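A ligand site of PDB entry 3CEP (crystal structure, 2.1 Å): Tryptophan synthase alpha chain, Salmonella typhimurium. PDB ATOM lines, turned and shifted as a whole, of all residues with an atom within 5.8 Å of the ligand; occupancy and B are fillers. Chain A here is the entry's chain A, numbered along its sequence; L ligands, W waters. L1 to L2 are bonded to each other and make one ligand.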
ATOM      1  N   PHE A  22      -1.010 -30.388   3.855  1.00  0.00           N
ATOM      2  CA  PHE A  22      -0.109 -31.505   4.197  1.00  0.00           C
ATOM      3  C   PHE A  22      -0.887 -32.772   4.555  1.00  0.00           C
ATOM      4  O   PHE A  22      -1.914 -32.710   5.225  1.00  0.00           O
ATOM      5  CB  PHE A  22       0.835 -31.135   5.350  1.00  0.00           C
ATOM      6  CG  PHE A  22       1.483 -32.337   6.011  1.00  0.00           C
ATOM      7  CD1 PHE A  22       0.862 -32.966   7.101  1.00  0.00           C
ATOM      8  CD2 PHE A  22       2.677 -32.839   5.545  1.00  0.00           C
ATOM      9  CE1 PHE A  22       1.444 -34.082   7.707  1.00  0.00           C
ATOM     10  CE2 PHE A  22       3.273 -33.956   6.147  1.00  0.00           C
ATOM     11  CZ  PHE A  22       2.650 -34.578   7.230  1.00  0.00           C
ATOM     12  N   GLU A  49       2.611 -30.776   0.503  1.00  0.00           N
ATOM     13  CA  GLU A  49       3.599 -31.204   1.475  1.00  0.00           C
ATOM     14  C   GLU A  49       3.202 -32.599   1.958  1.00  0.00           C
ATOM     15  O   GLU A  49       2.088 -32.806   2.425  1.00  0.00           O
ATOM     16  CB  GLU A  49       3.730 -30.212   2.643  1.00  0.00           C
ATOM     17  CG  GLU A  49       4.917 -30.505   3.551  1.00  0.00           C
ATOM     18  CD  GLU A  49       4.793 -29.822   4.914  1.00  0.00           C
ATOM     19  OE1 GLU A  49       5.264 -30.423   5.913  1.00  0.00           O
ATOM     20  OE2 GLU A  49       4.222 -28.716   4.989  1.00  0.00           O
ATOM     21  N   ALA A  59       8.530 -32.830  16.232  1.00  0.00           N
ATOM     22  CA  ALA A  59       7.934 -31.513  15.962  1.00  0.00           C
ATOM     23  C   ALA A  59       6.417 -31.586  15.764  1.00  0.00           C
ATOM     24  O   ALA A  59       5.793 -30.626  15.329  1.00  0.00           O
ATOM     25  CB  ALA A  59       8.627 -30.839  14.767  1.00  0.00           C
ATOM     26  N   ASP A  60       5.819 -32.718  16.134  1.00  0.00           N
ATOM     27  CA  ASP A  60       4.420 -32.976  15.846  1.00  0.00           C
ATOM     28  C   ASP A  60       3.570 -33.214  17.091  1.00  0.00           C
ATOM     29  O   ASP A  60       3.968 -33.941  17.998  1.00  0.00           O
ATOM     30  CB  ASP A  60       4.281 -34.163  14.888  1.00  0.00           C
ATOM     31  CG  ASP A  60       4.604 -33.778  13.462  1.00  0.00           C
ATOM     32  OD1 ASP A  60       3.875 -32.937  12.908  1.00  0.00           O
ATOM     33  OD2 ASP A  60       5.583 -34.327  12.893  1.00  0.00           O
ATOM     34  N   ILE A  64      -0.960 -35.290  14.047  1.00  0.00           N
ATOM     35  CA  ILE A  64      -0.032 -35.857  13.068  1.00  0.00           C
ATOM     36  C   ILE A  64       0.715 -37.071  13.631  1.00  0.00           C
ATOM     37  O   ILE A  64       1.056 -37.992  12.879  1.00  0.00           O
ATOM     38  CB  ILE A  64       0.918 -34.787  12.476  1.00  0.00           C
ATOM     39  CG1 ILE A  64       0.111 -33.779  11.650  1.00  0.00           C
ATOM     40  CG2 ILE A  64       1.958 -35.440  11.597  1.00  0.00           C
ATOM     41  CD1 ILE A  64       0.888 -32.552  11.193  1.00  0.00           C
ATOM     42  N   LEU A 100       8.175 -33.648   3.995  1.00  0.00           N
ATOM     43  CA  LEU A 100       8.537 -33.350   5.369  1.00  0.00           C
ATOM     44  C   LEU A 100       9.206 -34.589   5.928  1.00  0.00           C
ATOM     45  O   LEU A 100       8.583 -35.655   6.026  1.00  0.00           O
ATOM     46  CB  LEU A 100       7.331 -32.943   6.220  1.00  0.00           C
ATOM     47  CG  LEU A 100       7.605 -32.468   7.667  1.00  0.00           C
ATOM     48  CD1 LEU A 100       7.833 -33.626   8.679  1.00  0.00           C
ATOM     49  CD2 LEU A 100       8.752 -31.472   7.700  1.00  0.00           C
ATOM     50  N   TYR A 102      12.148 -36.291   8.876  1.00  0.00           N
ATOM     51  CA  TYR A 102      13.005 -36.213  10.062  1.00  0.00           C
ATOM     52  C   TYR A 102      14.398 -36.707   9.664  1.00  0.00           C
ATOM     53  O   TYR A 102      14.523 -37.549   8.778  1.00  0.00           O
ATOM     54  CB  TYR A 102      12.413 -36.986  11.244  1.00  0.00           C
ATOM     55  CG  TYR A 102      11.284 -36.196  11.867  1.00  0.00           C
ATOM     56  CD1 TYR A 102      11.529 -35.249  12.857  1.00  0.00           C
ATOM     57  CD2 TYR A 102       9.963 -36.349  11.416  1.00  0.00           C
ATOM     58  CE1 TYR A 102      10.513 -34.487  13.405  1.00  0.00           C
ATOM     59  CE2 TYR A 102       8.925 -35.590  11.967  1.00  0.00           C
ATOM     60  CZ  TYR A 102       9.207 -34.672  12.961  1.00  0.00           C
ATOM     61  OH  TYR A 102       8.185 -33.922  13.514  1.00  0.00           O
ATOM     62  N   LEU A 127      11.955 -30.690   3.475  1.00  0.00           N
ATOM     63  CA  LEU A 127      12.073 -30.016   4.760  1.00  0.00           C
ATOM     64  C   LEU A 127      12.499 -31.056   5.793  1.00  0.00           C
ATOM     65  O   LEU A 127      11.780 -32.021   6.020  1.00  0.00           O
ATOM     66  CB  LEU A 127      10.741 -29.403   5.174  1.00  0.00           C
ATOM     67  CG  LEU A 127      10.637 -28.152   6.049  1.00  0.00           C
ATOM     68  CD1 LEU A 127       9.252 -28.076   6.688  1.00  0.00           C
ATOM     69  CD2 LEU A 127      11.735 -28.020   7.121  1.00  0.00           C
ATOM     70  N   ALA A 129      12.783 -31.456   9.527  1.00  0.00           N
ATOM     71  CA  ALA A 129      12.259 -30.767  10.719  1.00  0.00           C
ATOM     72  C   ALA A 129      13.279 -30.556  11.849  1.00  0.00           C
ATOM     73  O   ALA A 129      13.258 -29.524  12.521  1.00  0.00           O
ATOM     74  CB  ALA A 129      11.030 -31.511  11.239  1.00  0.00           C
ATOM     75  N   ILE A 153      13.141 -23.518   8.016  1.00  0.00           N
ATOM     76  CA  ILE A 153      12.154 -22.821   8.823  1.00  0.00           C
ATOM     77  C   ILE A 153      12.702 -21.501   9.338  1.00  0.00           C
ATOM     78  O   ILE A 153      13.817 -21.431   9.864  1.00  0.00           O
ATOM     79  CB  ILE A 153      11.673 -23.695  10.002  1.00  0.00           C
ATOM     80  CG1 ILE A 153      10.849 -24.882   9.484  1.00  0.00           C
ATOM     81  CG2 ILE A 153      10.853 -22.873  10.992  1.00  0.00           C
ATOM     82  CD1 ILE A 153      10.594 -25.965  10.519  1.00  0.00           C
ATOM     83  N   TYR A 175       9.976 -21.590   4.839  1.00  0.00           N
ATOM     84  CA  TYR A 175       8.949 -22.014   5.785  1.00  0.00           C
ATOM     85  C   TYR A 175       8.873 -21.003   6.915  1.00  0.00           C
ATOM     86  O   TYR A 175       9.780 -20.907   7.758  1.00  0.00           O
ATOM     87  CB  TYR A 175       9.220 -23.420   6.345  1.00  0.00           C
ATOM     88  CG  TYR A 175       8.007 -24.062   7.009  1.00  0.00           C
ATOM     89  CD1 TYR A 175       7.487 -23.553   8.191  1.00  0.00           C
ATOM     90  CD2 TYR A 175       7.394 -25.185   6.436  1.00  0.00           C
ATOM     91  CE1 TYR A 175       6.371 -24.135   8.800  1.00  0.00           C
ATOM     92  CE2 TYR A 175       6.285 -25.780   7.045  1.00  0.00           C
ATOM     93  CZ  TYR A 175       5.778 -25.248   8.218  1.00  0.00           C
ATOM     94  OH  TYR A 175       4.680 -25.837   8.815  1.00  0.00           O
ATOM     95  N   ARG A 179       4.362 -19.818  14.975  1.00  0.00           N
ATOM     96  CA  ARG A 179       4.456 -19.852  16.452  1.00  0.00           C
ATOM     97  C   ARG A 179       5.435 -20.921  16.893  1.00  0.00           C
ATOM     98  O   ARG A 179       5.763 -21.833  16.125  1.00  0.00           O
ATOM     99  CB  ARG A 179       3.084 -20.152  17.084  1.00  0.00           C
ATOM    100  CG  ARG A 179       2.400 -21.425  16.554  1.00  0.00           C
ATOM    101  CD  ARG A 179       1.518 -22.085  17.598  1.00  0.00           C
ATOM    102  NE  ARG A 179       0.797 -23.233  17.046  1.00  0.00           N
ATOM    103  CZ  ARG A 179       1.260 -24.475  16.994  1.00  0.00           C
ATOM    104  NH1 ARG A 179       2.461 -24.775  17.484  1.00  0.00           N
ATOM    105  NH2 ARG A 179       0.522 -25.441  16.457  1.00  0.00           N
ATOM    106  N   VAL A 182       4.690 -27.300  18.741  1.00  0.00           N
ATOM    107  CA  VAL A 182       4.638 -28.385  17.774  1.00  0.00           C
ATOM    108  C   VAL A 182       3.377 -28.243  16.924  1.00  0.00           C
ATOM    109  O   VAL A 182       2.519 -27.423  17.225  1.00  0.00           O
ATOM    110  CB  VAL A 182       4.683 -29.790  18.457  1.00  0.00           C
ATOM    111  CG1 VAL A 182       5.970 -29.959  19.259  1.00  0.00           C
ATOM    112  CG2 VAL A 182       3.464 -30.020  19.350  1.00  0.00           C
ATOM    113  N   THR A 183       3.277 -29.035  15.861  1.00  0.00           N
ATOM    114  CA  THR A 183       2.125 -28.940  14.947  1.00  0.00           C
ATOM    115  C   THR A 183       0.813 -29.147  15.701  1.00  0.00           C
ATOM    116  O   THR A 183       0.759 -29.902  16.678  1.00  0.00           O
ATOM    117  CB  THR A 183       2.225 -29.955  13.778  1.00  0.00           C
ATOM    118  OG1 THR A 183       2.184 -31.293  14.292  1.00  0.00           O
ATOM    119  CG2 THR A 183       3.499 -29.744  12.980  1.00  0.00           C
ATOM    120  N   GLY A 184      -0.234 -28.455  15.259  1.00  0.00           N
ATOM    121  CA  GLY A 184      -1.532 -28.550  15.904  1.00  0.00           C
ATOM    122  C   GLY A 184      -2.500 -27.499  15.413  1.00  0.00           C
ATOM    123  O   GLY A 184      -2.203 -26.300  15.469  1.00  0.00           O
ATOM    124  N   ALA A 185      -3.649 -27.953  14.943  1.00  0.00           N
ATOM    125  CA  ALA A 185      -4.706 -27.092  14.415  1.00  0.00           C
ATOM    126  C   ALA A 185      -5.355 -26.196  15.488  1.00  0.00           C
ATOM    127  O   ALA A 185      -5.810 -25.093  15.194  1.00  0.00           O
ATOM    128  CB  ALA A 185      -5.772 -27.925  13.712  1.00  0.00           C
ATOM    129  N   GLY A 211       3.121 -21.649   8.167  1.00  0.00           N
ATOM    130  CA  GLY A 211       2.649 -22.956   8.631  1.00  0.00           C
ATOM    131  C   GLY A 211       2.709 -23.095  10.141  1.00  0.00           C
ATOM    132  O   GLY A 211       3.556 -22.464  10.802  1.00  0.00           O
ATOM    133  N   PHE A 212       1.816 -23.951  10.656  1.00  0.00           N
ATOM    134  CA  PHE A 212       1.563 -24.213  12.100  1.00  0.00           C
ATOM    135  C   PHE A 212       0.308 -23.513  12.581  1.00  0.00           C
ATOM    136  O   PHE A 212       0.264 -22.284  12.691  1.00  0.00           O
ATOM    137  CB  PHE A 212       2.749 -23.860  13.008  1.00  0.00           C
ATOM    138  CG  PHE A 212       3.766 -24.957  13.165  1.00  0.00           C
ATOM    139  CD1 PHE A 212       4.330 -25.579  12.045  1.00  0.00           C
ATOM    140  CD2 PHE A 212       4.198 -25.340  14.425  1.00  0.00           C
ATOM    141  CE1 PHE A 212       5.271 -26.572  12.197  1.00  0.00           C
ATOM    142  CE2 PHE A 212       5.139 -26.333  14.577  1.00  0.00           C
ATOM    143  CZ  PHE A 212       5.685 -26.948  13.469  1.00  0.00           C
ATOM    144  N   GLY A 213      -0.738 -24.297  12.865  1.00  0.00           N
ATOM    145  CA  GLY A 213      -1.976 -23.771  13.411  1.00  0.00           C
ATOM    146  C   GLY A 213      -2.940 -23.099  12.433  1.00  0.00           C
ATOM    147  O   GLY A 213      -3.914 -22.491  12.857  1.00  0.00           O
ATOM    148  N   ILE A 214      -2.673 -23.221  11.133  1.00  0.00           N
ATOM    149  CA  ILE A 214      -3.563 -22.670  10.113  1.00  0.00           C
ATOM    150  C   ILE A 214      -4.675 -23.679   9.826  1.00  0.00           C
ATOM    151  O   ILE A 214      -4.419 -24.749   9.266  1.00  0.00           O
ATOM    152  CB  ILE A 214      -2.810 -22.340   8.787  1.00  0.00           C
ATOM    153  CG1 ILE A 214      -1.501 -21.563   9.045  1.00  0.00           C
ATOM    154  CG2 ILE A 214      -3.729 -21.613   7.794  1.00  0.00           C
ATOM    155  CD1 ILE A 214      -1.663 -20.205   9.695  1.00  0.00           C
ATOM    156  N   ILE A 232       0.150 -22.936   4.715  1.00  0.00           N
ATOM    157  CA  ILE A 232       0.205 -24.383   4.788  1.00  0.00           C
ATOM    158  C   ILE A 232      -0.701 -24.856   5.911  1.00  0.00           C
ATOM    159  O   ILE A 232      -0.649 -24.329   7.024  1.00  0.00           O
ATOM    160  CB  ILE A 232       1.659 -24.893   5.066  1.00  0.00           C
ATOM    161  CG1 ILE A 232       2.648 -24.353   4.030  1.00  0.00           C
ATOM    162  CG2 ILE A 232       1.704 -26.432   5.092  1.00  0.00           C
ATOM    163  CD1 ILE A 232       4.086 -24.386   4.492  1.00  0.00           C
ATOM    164  N   SER A 233      -1.551 -25.833   5.612  1.00  0.00           N
ATOM    165  CA  SER A 233      -2.388 -26.453   6.625  1.00  0.00           C
ATOM    166  C   SER A 233      -2.112 -27.960   6.677  1.00  0.00           C
ATOM    167  O   SER A 233      -2.220 -28.645   5.653  1.00  0.00           O
ATOM    168  CB  SER A 233      -3.868 -26.196   6.330  1.00  0.00           C
ATOM    169  OG  SER A 233      -4.696 -26.780   7.320  1.00  0.00           O
ATOM    170  N   GLY A 234      -1.747 -28.442   7.856  1.00  0.00           N
ATOM    171  CA  GLY A 234      -1.453 -29.860   8.065  1.00  0.00           C
ATOM    172  C   GLY A 234      -2.467 -30.549   8.957  1.00  0.00           C
ATOM    173  O   GLY A 234      -3.314 -31.308   8.471  1.00  0.00           O
ATOM    174  N   SER A 235      -2.397 -30.276  10.257  1.00  0.00           N
ATOM    175  CA  SER A 235      -3.245 -30.934  11.250  1.00  0.00           C
ATOM    176  C   SER A 235      -4.749 -30.824  10.943  1.00  0.00           C
ATOM    177  O   SER A 235      -5.492 -31.785  11.165  1.00  0.00           O
ATOM    178  CB  SER A 235      -2.941 -30.411  12.665  1.00  0.00           C
ATOM    179  OG  SER A 235      -1.595 -30.660  13.021  1.00  0.00           O
ATOM    180  N   ALA A 236      -5.162 -29.675  10.424  1.00  0.00           N
ATOM    181  CA  ALA A 236      -6.560 -29.454  10.011  1.00  0.00           C
ATOM    182  C   ALA A 236      -6.998 -30.469   8.962  1.00  0.00           C
ATOM    183  O   ALA A 236      -8.076 -31.039   9.065  1.00  0.00           O
ATOM    184  CB  ALA A 236      -6.741 -28.040   9.490  1.00  0.00           C
HETATM  185  O1  LIG L   1       3.527 -28.230   7.401  1.00  0.00           O
HETATM  186  C1  LIG L   1       3.613 -28.872   8.554  1.00  0.00           C
HETATM  187  C2  LIG L   1       2.336 -28.877   9.299  1.00  0.00           C
HETATM  188  O2  LIG L   1       2.018 -30.024   9.881  1.00  0.00           O
HETATM  189  C3  LIG L   1       2.315 -27.861  10.332  1.00  0.00           C
HETATM  190  O3  LIG L   1       1.058 -27.137  10.301  1.00  0.00           O
HETATM  191  O4  LIG L   1       0.127 -27.162  12.595  1.00  0.00           O
HETATM  192  O5  LIG L   1      -0.093 -29.236  11.169  1.00  0.00           O
HETATM  193  O6  LIG L   1      -1.339 -27.142  10.534  1.00  0.00           O
HETATM  194  P1  LIG L   1      -0.132 -27.726  11.228  1.00  0.00           P
HETATM  195  N1  LG2 L   2       4.464 -30.095   8.383  1.00  0.00           N
HETATM  196  C1  LG2 L   2       3.858 -31.408   8.748  1.00  0.00           C
HETATM  197  C2  LG2 L   2       4.601 -31.980   9.990  1.00  0.00           C
HETATM  198  C3  LG2 L   2       5.650 -30.923  10.198  1.00  0.00           C
HETATM  199  C4  LG2 L   2       6.639 -30.904  11.158  1.00  0.00           C
HETATM  200  C5  LG2 L   2       7.533 -29.808  11.159  1.00  0.00           C
HETATM  201  C6  LG2 L   2       7.410 -28.771  10.214  1.00  0.00           C
HETATM  202  C7  LG2 L   2       6.399 -28.809   9.241  1.00  0.00           C
HETATM  203  C8  LG2 L   2       5.524 -29.903   9.251  1.00  0.00           C
HETATM  204  O   HOH W   1      -0.378 -24.813   9.531  1.00  0.00           O
HETATM  205  O   HOH W   2      -3.942 -27.103  10.855  1.00  0.00           O
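N of Gly 184 sits at hydrogen-bond distance from OG of Ser 235 (3.4 Å).
NH2 of Arg 179 sits at hydrogen-bond distance from O of Gly 184 (3.0 Å).
The side-chain hydroxyl (OG1) of Thr 183 lies within hydrogen-bond range of the side-chain carboxylate (OD1) of Asp 60, at 2.7 Å.
OD2 of Asp 60 lies within hydrogen-bond range of OH of Tyr 102 (2.7 Å).
The backbone NH of Thr 183 sits at hydrogen-bond distance from the backbone carbonyl oxygen of Ala 59, at 3.0 Å.
O of Ser 233 is in hydrogen-bond range of N of Phe 22 (2.8 Å).
OH of Tyr 102 is in hydrogen-bond range of N of Ala 59 (2.9 Å).
Water W2 lies within hydrogen-bond range of O6 of LIG L1 (2.6 Å), O of Ile 214 (2.9 Å) and N of Ala 236 (2.9 Å).
The side-chain carboxylate (OE2) of Glu 49 sits at hydrogen-bond distance from an oxygen (O1) of LIG L1, at 2.6 Å.
The backbone NH (N) of Ser 235 is in hydrogen-bond range of an oxygen (O5) of LIG L1, 2.7 Å away.
An oxygen (O5) of LIG L1 sits at hydrogen-bond distance from the side-chain hydroxyl of Ser 235, 2.8 Å away.
The backbone NH of Gly 184 lies within hydrogen-bond range of an oxygen (O4) of LIG L1 (3.0 Å).
An oxygen (O6) of LIG L1 lies within hydrogen-bond range of the backbone NH of Gly 234, 3.0 Å away.
N of Gly 213 is in hydrogen-bond range of O4 of LIG L1, 3.0 Å away.
OH of Tyr 175 sits at hydrogen-bond distance from O1 of LIG L1, 3.0 Å away.
O3 of LIG L1 is in hydrogen-bond range of N of Phe 212 (3.3 Å).
CE2 of Phe 22 touches C1 of LG2 L2 (3.7 Å).
CB of Ala 59 touches C5 of LG2 L2, at 3.9 Å.
OD1 of Asp 60 touches C2 of LG2 L2, 3.2 Å away.
CD1 of Ile 64 touches O2 of LIG L1 (3.1 Å).
CG of Leu 100 touches C3 of LG2 L2 (3.6 Å).
CD1 of Leu 127 touches C7 of LG2 L2, 3.9 Å away.
CB of Ala 129 touches C5 of LG2 L2 (3.9 Å).
CG2 of Thr 183 touches O2 of LIG L1, at 3.4 Å.
Ile 232 touches the ligand.
Within 4 Å of the ligand: Phe 22, Glu 49, Ala 59, Asp 60, Ile 64, Leu 100, Leu 127, Ala 129, Tyr 175, Thr 183, Gly 184, Phe 212, Gly 213, Ile 232, Gly 234 and Ser 235.
The nearest printed residue that does not touch the ligand is Ser 233 (4.02 Å).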
